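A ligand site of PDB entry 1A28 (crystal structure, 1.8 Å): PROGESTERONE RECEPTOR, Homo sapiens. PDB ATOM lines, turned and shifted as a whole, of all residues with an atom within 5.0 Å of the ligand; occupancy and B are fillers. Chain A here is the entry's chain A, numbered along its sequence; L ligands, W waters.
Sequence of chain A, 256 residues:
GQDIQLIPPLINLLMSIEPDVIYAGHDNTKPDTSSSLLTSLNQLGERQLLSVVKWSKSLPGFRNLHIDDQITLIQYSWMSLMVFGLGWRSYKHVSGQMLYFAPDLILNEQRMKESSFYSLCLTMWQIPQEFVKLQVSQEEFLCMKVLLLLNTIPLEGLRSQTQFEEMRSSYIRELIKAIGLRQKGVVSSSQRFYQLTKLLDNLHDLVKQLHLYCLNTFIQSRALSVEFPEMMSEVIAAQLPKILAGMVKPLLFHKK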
ATOM      1  N   LEU A  38     -10.078 -25.538  23.259  1.00  0.00           N
ATOM      2  CA  LEU A  38     -11.201 -24.919  23.971  1.00  0.00           C
ATOM      3  C   LEU A  38     -10.730 -24.036  25.082  1.00  0.00           C
ATOM      4  O   LEU A  38     -11.265 -22.946  25.278  1.00  0.00           O
ATOM      5  CB  LEU A  38     -12.147 -25.973  24.496  1.00  0.00           C
ATOM      6  CG  LEU A  38     -12.792 -26.799  23.379  1.00  0.00           C
ATOM      7  CD1 LEU A  38     -13.617 -27.927  23.977  1.00  0.00           C
ATOM      8  CD2 LEU A  38     -13.655 -25.889  22.517  1.00  0.00           C
ATOM      9  N   LEU A  41      -9.599 -20.932  23.570  1.00  0.00           N
ATOM     10  CA  LEU A  41     -10.701 -20.099  23.101  1.00  0.00           C
ATOM     11  C   LEU A  41     -11.395 -19.439  24.298  1.00  0.00           C
ATOM     12  O   LEU A  41     -11.914 -18.324  24.180  1.00  0.00           O
ATOM     13  CB  LEU A  41     -11.708 -20.927  22.312  1.00  0.00           C
ATOM     14  CG  LEU A  41     -11.232 -21.376  20.926  1.00  0.00           C
ATOM     15  CD1 LEU A  41     -12.238 -22.339  20.362  1.00  0.00           C
ATOM     16  CD2 LEU A  41     -11.065 -20.171  20.005  1.00  0.00           C
ATOM     17  N   ASN A  42     -11.406 -20.124  25.433  1.00  0.00           N
ATOM     18  CA  ASN A  42     -12.016 -19.507  26.635  1.00  0.00           C
ATOM     19  C   ASN A  42     -11.157 -18.353  27.142  1.00  0.00           C
ATOM     20  O   ASN A  42     -11.688 -17.363  27.642  1.00  0.00           O
ATOM     21  CB  ASN A  42     -12.206 -20.519  27.778  1.00  0.00           C
ATOM     22  CG  ASN A  42     -13.358 -21.467  27.539  1.00  0.00           C
ATOM     23  OD1 ASN A  42     -14.336 -21.146  26.839  1.00  0.00           O
ATOM     24  ND2 ASN A  42     -13.285 -22.639  28.163  1.00  0.00           N
ATOM     25  N   LEU A  44      -9.343 -16.465  25.262  1.00  0.00           N
ATOM     26  CA  LEU A  44      -9.630 -15.396  24.317  1.00  0.00           C
ATOM     27  C   LEU A  44     -10.969 -14.758  24.697  1.00  0.00           C
ATOM     28  O   LEU A  44     -11.115 -13.538  24.717  1.00  0.00           O
ATOM     29  CB  LEU A  44      -9.682 -15.940  22.883  1.00  0.00           C
ATOM     30  CG  LEU A  44     -10.039 -14.921  21.803  1.00  0.00           C
ATOM     31  CD1 LEU A  44      -8.989 -13.794  21.780  1.00  0.00           C
ATOM     32  CD2 LEU A  44     -10.115 -15.649  20.433  1.00  0.00           C
ATOM     33  N   GLY A  45     -11.949 -15.600  25.016  1.00  0.00           N
ATOM     34  CA  GLY A  45     -13.282 -15.135  25.402  1.00  0.00           C
ATOM     35  C   GLY A  45     -13.212 -14.234  26.623  1.00  0.00           C
ATOM     36  O   GLY A  45     -13.918 -13.227  26.714  1.00  0.00           O
ATOM     37  N   GLN A  48     -11.945 -10.973  25.467  1.00  0.00           N
ATOM     38  CA  GLN A  48     -12.928 -10.251  24.689  1.00  0.00           C
ATOM     39  C   GLN A  48     -14.066  -9.730  25.560  1.00  0.00           C
ATOM     40  O   GLN A  48     -14.662  -8.698  25.258  1.00  0.00           O
ATOM     41  CB  GLN A  48     -13.495 -11.121  23.555  1.00  0.00           C
ATOM     42  CG  GLN A  48     -12.441 -11.361  22.475  1.00  0.00           C
ATOM     43  CD  GLN A  48     -12.991 -12.057  21.246  1.00  0.00           C
ATOM     44  OE1 GLN A  48     -12.240 -12.363  20.306  1.00  0.00           O
ATOM     45  NE2 GLN A  48     -14.290 -12.306  21.247  1.00  0.00           N
ATOM     46  N   TRP A  78     -23.203 -11.397  25.334  1.00  0.00           N
ATOM     47  CA  TRP A  78     -21.776 -11.583  25.075  1.00  0.00           C
ATOM     48  C   TRP A  78     -21.476 -12.622  23.985  1.00  0.00           C
ATOM     49  O   TRP A  78     -20.648 -12.375  23.125  1.00  0.00           O
ATOM     50  CB  TRP A  78     -20.992 -11.923  26.349  1.00  0.00           C
ATOM     51  CG  TRP A  78     -21.346 -13.233  26.973  1.00  0.00           C
ATOM     52  CD1 TRP A  78     -22.380 -13.488  27.838  1.00  0.00           C
ATOM     53  CD2 TRP A  78     -20.697 -14.484  26.746  1.00  0.00           C
ATOM     54  NE1 TRP A  78     -22.411 -14.829  28.161  1.00  0.00           N
ATOM     55  CE2 TRP A  78     -21.381 -15.460  27.509  1.00  0.00           C
ATOM     56  CE3 TRP A  78     -19.595 -14.871  25.979  1.00  0.00           C
ATOM     57  CZ2 TRP A  78     -21.004 -16.815  27.521  1.00  0.00           C
ATOM     58  CZ3 TRP A  78     -19.217 -16.216  25.990  1.00  0.00           C
ATOM     59  CH2 TRP A  78     -19.917 -17.169  26.749  1.00  0.00           C
ATOM     60  N   MET A  79     -22.145 -13.774  24.028  1.00  0.00           N
ATOM     61  CA  MET A  79     -21.889 -14.820  23.024  1.00  0.00           C
ATOM     62  C   MET A  79     -22.228 -14.345  21.621  1.00  0.00           C
ATOM     63  O   MET A  79     -21.469 -14.602  20.667  1.00  0.00           O
ATOM     64  CB  MET A  79     -22.703 -16.084  23.332  1.00  0.00           C
ATOM     65  CG  MET A  79     -22.404 -17.225  22.362  1.00  0.00           C
ATOM     66  SD  MET A  79     -20.787 -18.037  22.661  1.00  0.00           S
ATOM     67  CE  MET A  79     -21.219 -19.027  24.167  1.00  0.00           C
ATOM     68  N   MET A  82     -19.631 -11.806  20.427  1.00  0.00           N
ATOM     69  CA  MET A  82     -18.361 -12.428  20.118  1.00  0.00           C
ATOM     70  C   MET A  82     -18.400 -13.286  18.857  1.00  0.00           C
ATOM     71  O   MET A  82     -17.423 -13.268  18.087  1.00  0.00           O
ATOM     72  CB  MET A  82     -17.868 -13.236  21.318  1.00  0.00           C
ATOM     73  CG  MET A  82     -17.475 -12.327  22.498  1.00  0.00           C
ATOM     74  SD  MET A  82     -16.786 -13.233  23.873  1.00  0.00           S
ATOM     75  CE  MET A  82     -16.769 -11.945  25.142  1.00  0.00           C
ATOM     76  N   VAL A  83     -19.473 -14.032  18.629  1.00  0.00           N
ATOM     77  CA  VAL A  83     -19.531 -14.843  17.411  1.00  0.00           C
ATOM     78  C   VAL A  83     -19.720 -13.931  16.180  1.00  0.00           C
ATOM     79  O   VAL A  83     -19.235 -14.237  15.095  1.00  0.00           O
ATOM     80  CB  VAL A  83     -20.667 -15.903  17.458  1.00  0.00           C
ATOM     81  CG1 VAL A  83     -22.044 -15.252  17.396  1.00  0.00           C
ATOM     82  CG2 VAL A  83     -20.512 -16.885  16.293  1.00  0.00           C
ATOM     83  N   LEU A  86     -16.406 -12.606  15.411  1.00  0.00           N
ATOM     84  CA  LEU A  86     -15.642 -13.662  14.775  1.00  0.00           C
ATOM     85  C   LEU A  86     -15.999 -13.687  13.285  1.00  0.00           C
ATOM     86  O   LEU A  86     -15.126 -13.843  12.418  1.00  0.00           O
ATOM     87  CB  LEU A  86     -16.003 -15.011  15.402  1.00  0.00           C
ATOM     88  CG  LEU A  86     -15.645 -16.280  14.613  1.00  0.00           C
ATOM     89  CD1 LEU A  86     -14.141 -16.442  14.555  1.00  0.00           C
ATOM     90  CD2 LEU A  86     -16.297 -17.479  15.290  1.00  0.00           C
ATOM     91  N   ARG A  89     -14.285 -10.703  11.483  1.00  0.00           N
ATOM     92  CA  ARG A  89     -12.855 -10.885  11.285  1.00  0.00           C
ATOM     93  C   ARG A  89     -12.557 -11.961  10.239  1.00  0.00           C
ATOM     94  O   ARG A  89     -11.641 -11.824   9.440  1.00  0.00           O
ATOM     95  CB  ARG A  89     -12.155 -11.270  12.604  1.00  0.00           C
ATOM     96  CG  ARG A  89     -12.179 -10.162  13.682  1.00  0.00           C
ATOM     97  CD  ARG A  89     -11.313 -10.582  14.873  1.00  0.00           C
ATOM     98  NE  ARG A  89     -11.812 -11.774  15.558  1.00  0.00           N
ATOM     99  CZ  ARG A  89     -12.786 -11.781  16.469  1.00  0.00           C
ATOM    100  NH1 ARG A  89     -13.358 -10.643  16.827  1.00  0.00           N
ATOM    101  NH2 ARG A  89     -13.169 -12.919  17.032  1.00  0.00           N
ATOM    102  N   PHE A 101     -10.466 -16.429  14.905  1.00  0.00           N
ATOM    103  CA  PHE A 101     -10.765 -16.098  16.294  1.00  0.00           C
ATOM    104  C   PHE A 101      -9.867 -14.961  16.787  1.00  0.00           C
ATOM    105  O   PHE A 101     -10.317 -14.032  17.454  1.00  0.00           O
ATOM    106  CB  PHE A 101     -10.608 -17.344  17.189  1.00  0.00           C
ATOM    107  CG  PHE A 101     -11.683 -18.362  16.986  1.00  0.00           C
ATOM    108  CD1 PHE A 101     -11.560 -19.364  16.031  1.00  0.00           C
ATOM    109  CD2 PHE A 101     -12.859 -18.300  17.733  1.00  0.00           C
ATOM    110  CE1 PHE A 101     -12.600 -20.285  15.824  1.00  0.00           C
ATOM    111  CE2 PHE A 101     -13.897 -19.212  17.525  1.00  0.00           C
ATOM    112  CZ  PHE A 101     -13.774 -20.203  16.580  1.00  0.00           C
ATOM    113  N   LEU A 120     -19.977 -27.429  15.528  1.00  0.00           N
ATOM    114  CA  LEU A 120     -20.296 -26.123  16.075  1.00  0.00           C
ATOM    115  C   LEU A 120     -19.653 -25.027  15.214  1.00  0.00           C
ATOM    116  O   LEU A 120     -20.229 -23.959  15.022  1.00  0.00           O
ATOM    117  CB  LEU A 120     -19.815 -25.988  17.520  1.00  0.00           C
ATOM    118  CG  LEU A 120     -20.367 -24.737  18.225  1.00  0.00           C
ATOM    119  CD1 LEU A 120     -21.858 -24.910  18.428  1.00  0.00           C
ATOM    120  CD2 LEU A 120     -19.695 -24.518  19.554  1.00  0.00           C
ATOM    121  N   MET A 124     -21.092 -21.705  13.267  1.00  0.00           N
ATOM    122  CA  MET A 124     -20.532 -20.372  13.386  1.00  0.00           C
ATOM    123  C   MET A 124     -20.190 -19.826  12.002  1.00  0.00           C
ATOM    124  O   MET A 124     -20.382 -18.651  11.727  1.00  0.00           O
ATOM    125  CB  MET A 124     -19.270 -20.388  14.265  1.00  0.00           C
ATOM    126  CG  MET A 124     -19.564 -20.732  15.738  1.00  0.00           C
ATOM    127  SD  MET A 124     -18.103 -20.482  16.779  1.00  0.00           S
ATOM    128  CE  MET A 124     -17.146 -21.895  16.373  1.00  0.00           C
ATOM    129  N   LEU A 210     -24.639 -22.378  20.342  1.00  0.00           N
ATOM    130  CA  LEU A 210     -23.388 -22.033  21.004  1.00  0.00           C
ATOM    131  C   LEU A 210     -23.609 -22.019  22.534  1.00  0.00           C
ATOM    132  O   LEU A 210     -22.774 -22.506  23.292  1.00  0.00           O
ATOM    133  CB  LEU A 210     -22.893 -20.673  20.525  1.00  0.00           C
ATOM    134  CG  LEU A 210     -22.637 -20.477  19.031  1.00  0.00           C
ATOM    135  CD1 LEU A 210     -21.977 -19.112  18.836  1.00  0.00           C
ATOM    136  CD2 LEU A 210     -21.719 -21.569  18.499  1.00  0.00           C
ATOM    137  N   TYR A 213     -23.745 -25.666  23.817  1.00  0.00           N
ATOM    138  CA  TYR A 213     -22.425 -26.305  23.790  1.00  0.00           C
ATOM    139  C   TYR A 213     -21.550 -25.765  24.943  1.00  0.00           C
ATOM    140  O   TYR A 213     -20.857 -26.508  25.656  1.00  0.00           O
ATOM    141  CB  TYR A 213     -21.760 -26.051  22.423  1.00  0.00           C
ATOM    142  CG  TYR A 213     -20.518 -26.887  22.171  1.00  0.00           C
ATOM    143  CD1 TYR A 213     -19.315 -26.607  22.823  1.00  0.00           C
ATOM    144  CD2 TYR A 213     -20.563 -27.979  21.305  1.00  0.00           C
ATOM    145  CE1 TYR A 213     -18.183 -27.383  22.612  1.00  0.00           C
ATOM    146  CE2 TYR A 213     -19.444 -28.774  21.095  1.00  0.00           C
ATOM    147  CZ  TYR A 213     -18.258 -28.470  21.752  1.00  0.00           C
ATOM    148  OH  TYR A 213     -17.137 -29.243  21.550  1.00  0.00           O
ATOM    149  N   CYS A 214     -21.606 -24.454  25.148  1.00  0.00           N
ATOM    150  CA  CYS A 214     -20.835 -23.803  26.207  1.00  0.00           C
ATOM    151  C   CYS A 214     -21.222 -24.301  27.601  1.00  0.00           C
ATOM    152  O   CYS A 214     -20.378 -24.674  28.410  1.00  0.00           O
ATOM    153  CB  CYS A 214     -21.035 -22.289  26.112  1.00  0.00           C
ATOM    154  SG  CYS A 214     -20.137 -21.339  27.372  1.00  0.00           S
ATOM    155  N   THR A 217     -20.064 -27.908  28.123  1.00  0.00           N
ATOM    156  CA  THR A 217     -18.628 -28.000  28.332  1.00  0.00           C
ATOM    157  C   THR A 217     -18.226 -27.434  29.687  1.00  0.00           C
ATOM    158  O   THR A 217     -17.291 -27.915  30.315  1.00  0.00           O
ATOM    159  CB  THR A 217     -17.864 -27.235  27.214  1.00  0.00           C
ATOM    160  OG1 THR A 217     -18.228 -27.799  25.955  1.00  0.00           O
ATOM    161  CG2 THR A 217     -16.366 -27.348  27.403  1.00  0.00           C
ATOM    162  N   VAL A 226     -11.101 -28.783  30.375  1.00  0.00           N
ATOM    163  CA  VAL A 226     -11.249 -27.455  29.788  1.00  0.00           C
ATOM    164  C   VAL A 226     -11.376 -26.411  30.889  1.00  0.00           C
ATOM    165  O   VAL A 226     -12.252 -26.498  31.749  1.00  0.00           O
ATOM    166  CB  VAL A 226     -12.498 -27.382  28.875  1.00  0.00           C
ATOM    167  CG1 VAL A 226     -12.666 -25.957  28.316  1.00  0.00           C
ATOM    168  CG2 VAL A 226     -12.358 -28.391  27.721  1.00  0.00           C
ATOM    169  N   PHE A 228     -12.173 -22.633  32.341  1.00  0.00           N
ATOM    170  CA  PHE A 228     -12.952 -21.429  32.060  1.00  0.00           C
ATOM    171  C   PHE A 228     -12.469 -20.376  33.036  1.00  0.00           C
ATOM    172  O   PHE A 228     -12.419 -20.640  34.241  1.00  0.00           O
ATOM    173  CB  PHE A 228     -14.471 -21.626  32.302  1.00  0.00           C
ATOM    174  CG  PHE A 228     -15.166 -22.450  31.249  1.00  0.00           C
ATOM    175  CD1 PHE A 228     -15.018 -23.825  31.203  1.00  0.00           C
ATOM    176  CD2 PHE A 228     -15.966 -21.841  30.292  1.00  0.00           C
ATOM    177  CE1 PHE A 228     -15.642 -24.583  30.223  1.00  0.00           C
ATOM    178  CE2 PHE A 228     -16.605 -22.577  29.298  1.00  0.00           C
ATOM    179  CZ  PHE A 228     -16.439 -23.954  29.265  1.00  0.00           C
ATOM    180  N   MET A 232     -15.744 -15.147  32.674  1.00  0.00           N
ATOM    181  CA  MET A 232     -16.584 -15.917  31.769  1.00  0.00           C
ATOM    182  C   MET A 232     -17.416 -16.908  32.566  1.00  0.00           C
ATOM    183  O   MET A 232     -18.578 -17.140  32.249  1.00  0.00           O
ATOM    184  CB  MET A 232     -15.732 -16.660  30.751  1.00  0.00           C
ATOM    185  CG  MET A 232     -16.534 -17.327  29.680  1.00  0.00           C
ATOM    186  SD  MET A 232     -15.403 -17.987  28.426  1.00  0.00           S
ATOM    187  CE  MET A 232     -16.566 -18.750  27.358  1.00  0.00           C
HETATM  188  C1  LIG L   1     -14.233 -16.905  21.853  1.00  0.00           C
HETATM  189  C2  LIG L   1     -13.981 -15.496  21.258  1.00  0.00           C
HETATM  190  C3  LIG L   1     -14.548 -15.433  19.835  1.00  0.00           C
HETATM  191  O1  LIG L   1     -14.020 -14.683  19.002  1.00  0.00           O
HETATM  192  C4  LIG L   1     -15.751 -16.188  19.500  1.00  0.00           C
HETATM  193  C5  LIG L   1     -16.324 -16.999  20.374  1.00  0.00           C
HETATM  194  C6  LIG L   1     -17.639 -17.670  19.977  1.00  0.00           C
HETATM  195  C7  LIG L   1     -17.645 -19.175  20.319  1.00  0.00           C
HETATM  196  C8  LIG L   1     -17.218 -19.478  21.777  1.00  0.00           C
HETATM  197  C9  LIG L   1     -15.781 -18.899  22.005  1.00  0.00           C
HETATM  198  C10 LIG L   1     -15.714 -17.343  21.789  1.00  0.00           C
HETATM  199  C11 LIG L   1     -15.215 -19.310  23.380  1.00  0.00           C
HETATM  200  C12 LIG L   1     -15.260 -20.849  23.598  1.00  0.00           C
HETATM  201  C13 LIG L   1     -16.702 -21.392  23.437  1.00  0.00           C
HETATM  202  C14 LIG L   1     -17.147 -20.995  21.987  1.00  0.00           C
HETATM  203  C15 LIG L   1     -18.444 -21.808  21.758  1.00  0.00           C
HETATM  204  C16 LIG L   1     -18.124 -23.174  22.462  1.00  0.00           C
HETATM  205  C17 LIG L   1     -16.823 -22.944  23.313  1.00  0.00           C
HETATM  206  C18 LIG L   1     -17.672 -20.877  24.562  1.00  0.00           C
HETATM  207  C19 LIG L   1     -16.584 -16.544  22.850  1.00  0.00           C
HETATM  208  C20 LIG L   1     -16.782 -23.715  24.644  1.00  0.00           C
HETATM  209  O2  LIG L   1     -17.766 -24.274  25.068  1.00  0.00           O
HETATM  210  C21 LIG L   1     -15.499 -23.772  25.408  1.00  0.00           C
HETATM  211  O   HOH W   1     -15.224 -11.840  18.758  1.00  0.00           O
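An oxygen (O1) of the ligand is in hydrogen-bond range of the guanidinium group of Arg 89, at 2.8 Å. The side-chain amide oxygen (OE1) of Gln 48 lies close to an oxygen (O1) of the ligand, at 3.2 Å.
The guanidinium group of Arg 89 is in hydrogen-bond range of the side-chain amide oxygen of Gln 48 (3.4 Å). The guanidinium group (NH2) of Arg 89 is in hydrogen-bond range of the backbone carbonyl oxygen (O) of Phe 101 (3.1 Å). The side-chain sulfur (SD) of Met 82 sits close to the side-chain amide nitrogen (NE2) of Gln 48. OD1 of Asn 42 sits close to SD of Met 232, 3.7 Å away. The backbone carbonyl oxygen of Tyr 213 is in hydrogen-bond range of the side-chain hydroxyl of Thr 217, at 2.9 Å.
Leu 41 touches the ligand (O to C11, 3.5 Å). Asn 42 touches the ligand (OD1 to C21, 3.2 Å). Leu 44 touches the ligand. SD of Met 79 touches C8 of the ligand (3.9 Å). SD of Met 82 touches C19 of the ligand, 3.5 Å away. Phe 101 touches the ligand (CD2 to C3, 3.9 Å). Leu 120 touches the ligand (CD2 to C16, 3.6 Å). SD of Met 124 touches C7 of the ligand, 3.8 Å away. CD1 of Tyr 213 touches O2 of the ligand, 3.6 Å away. Cys 214 touches the ligand. CB of Thr 217 touches O2 of the ligand, at 3.7 Å. Phe 228 touches the ligand (CZ to C21, 3.97 Å). CE of Met 232 touches C18 of the ligand (3.7 Å). Hydrophobic or aromatic side chains that line the ligand: Leu 41, Leu 44, Met 79, Met 82, Phe 101, Leu 120, Met 124, Tyr 213, Phe 228 and Met 232. The nearest printed residue that does not touch the ligand is Leu 38 (4.03 Å).
Water W1 lies within hydrogen-bond range of the side-chain amide nitrogen (NE2) of Gln 48, the backbone carbonyl oxygen (O) of Met 82, the guanidinium group (NH2) of Arg 89 and an oxygen (O1) of the ligand.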
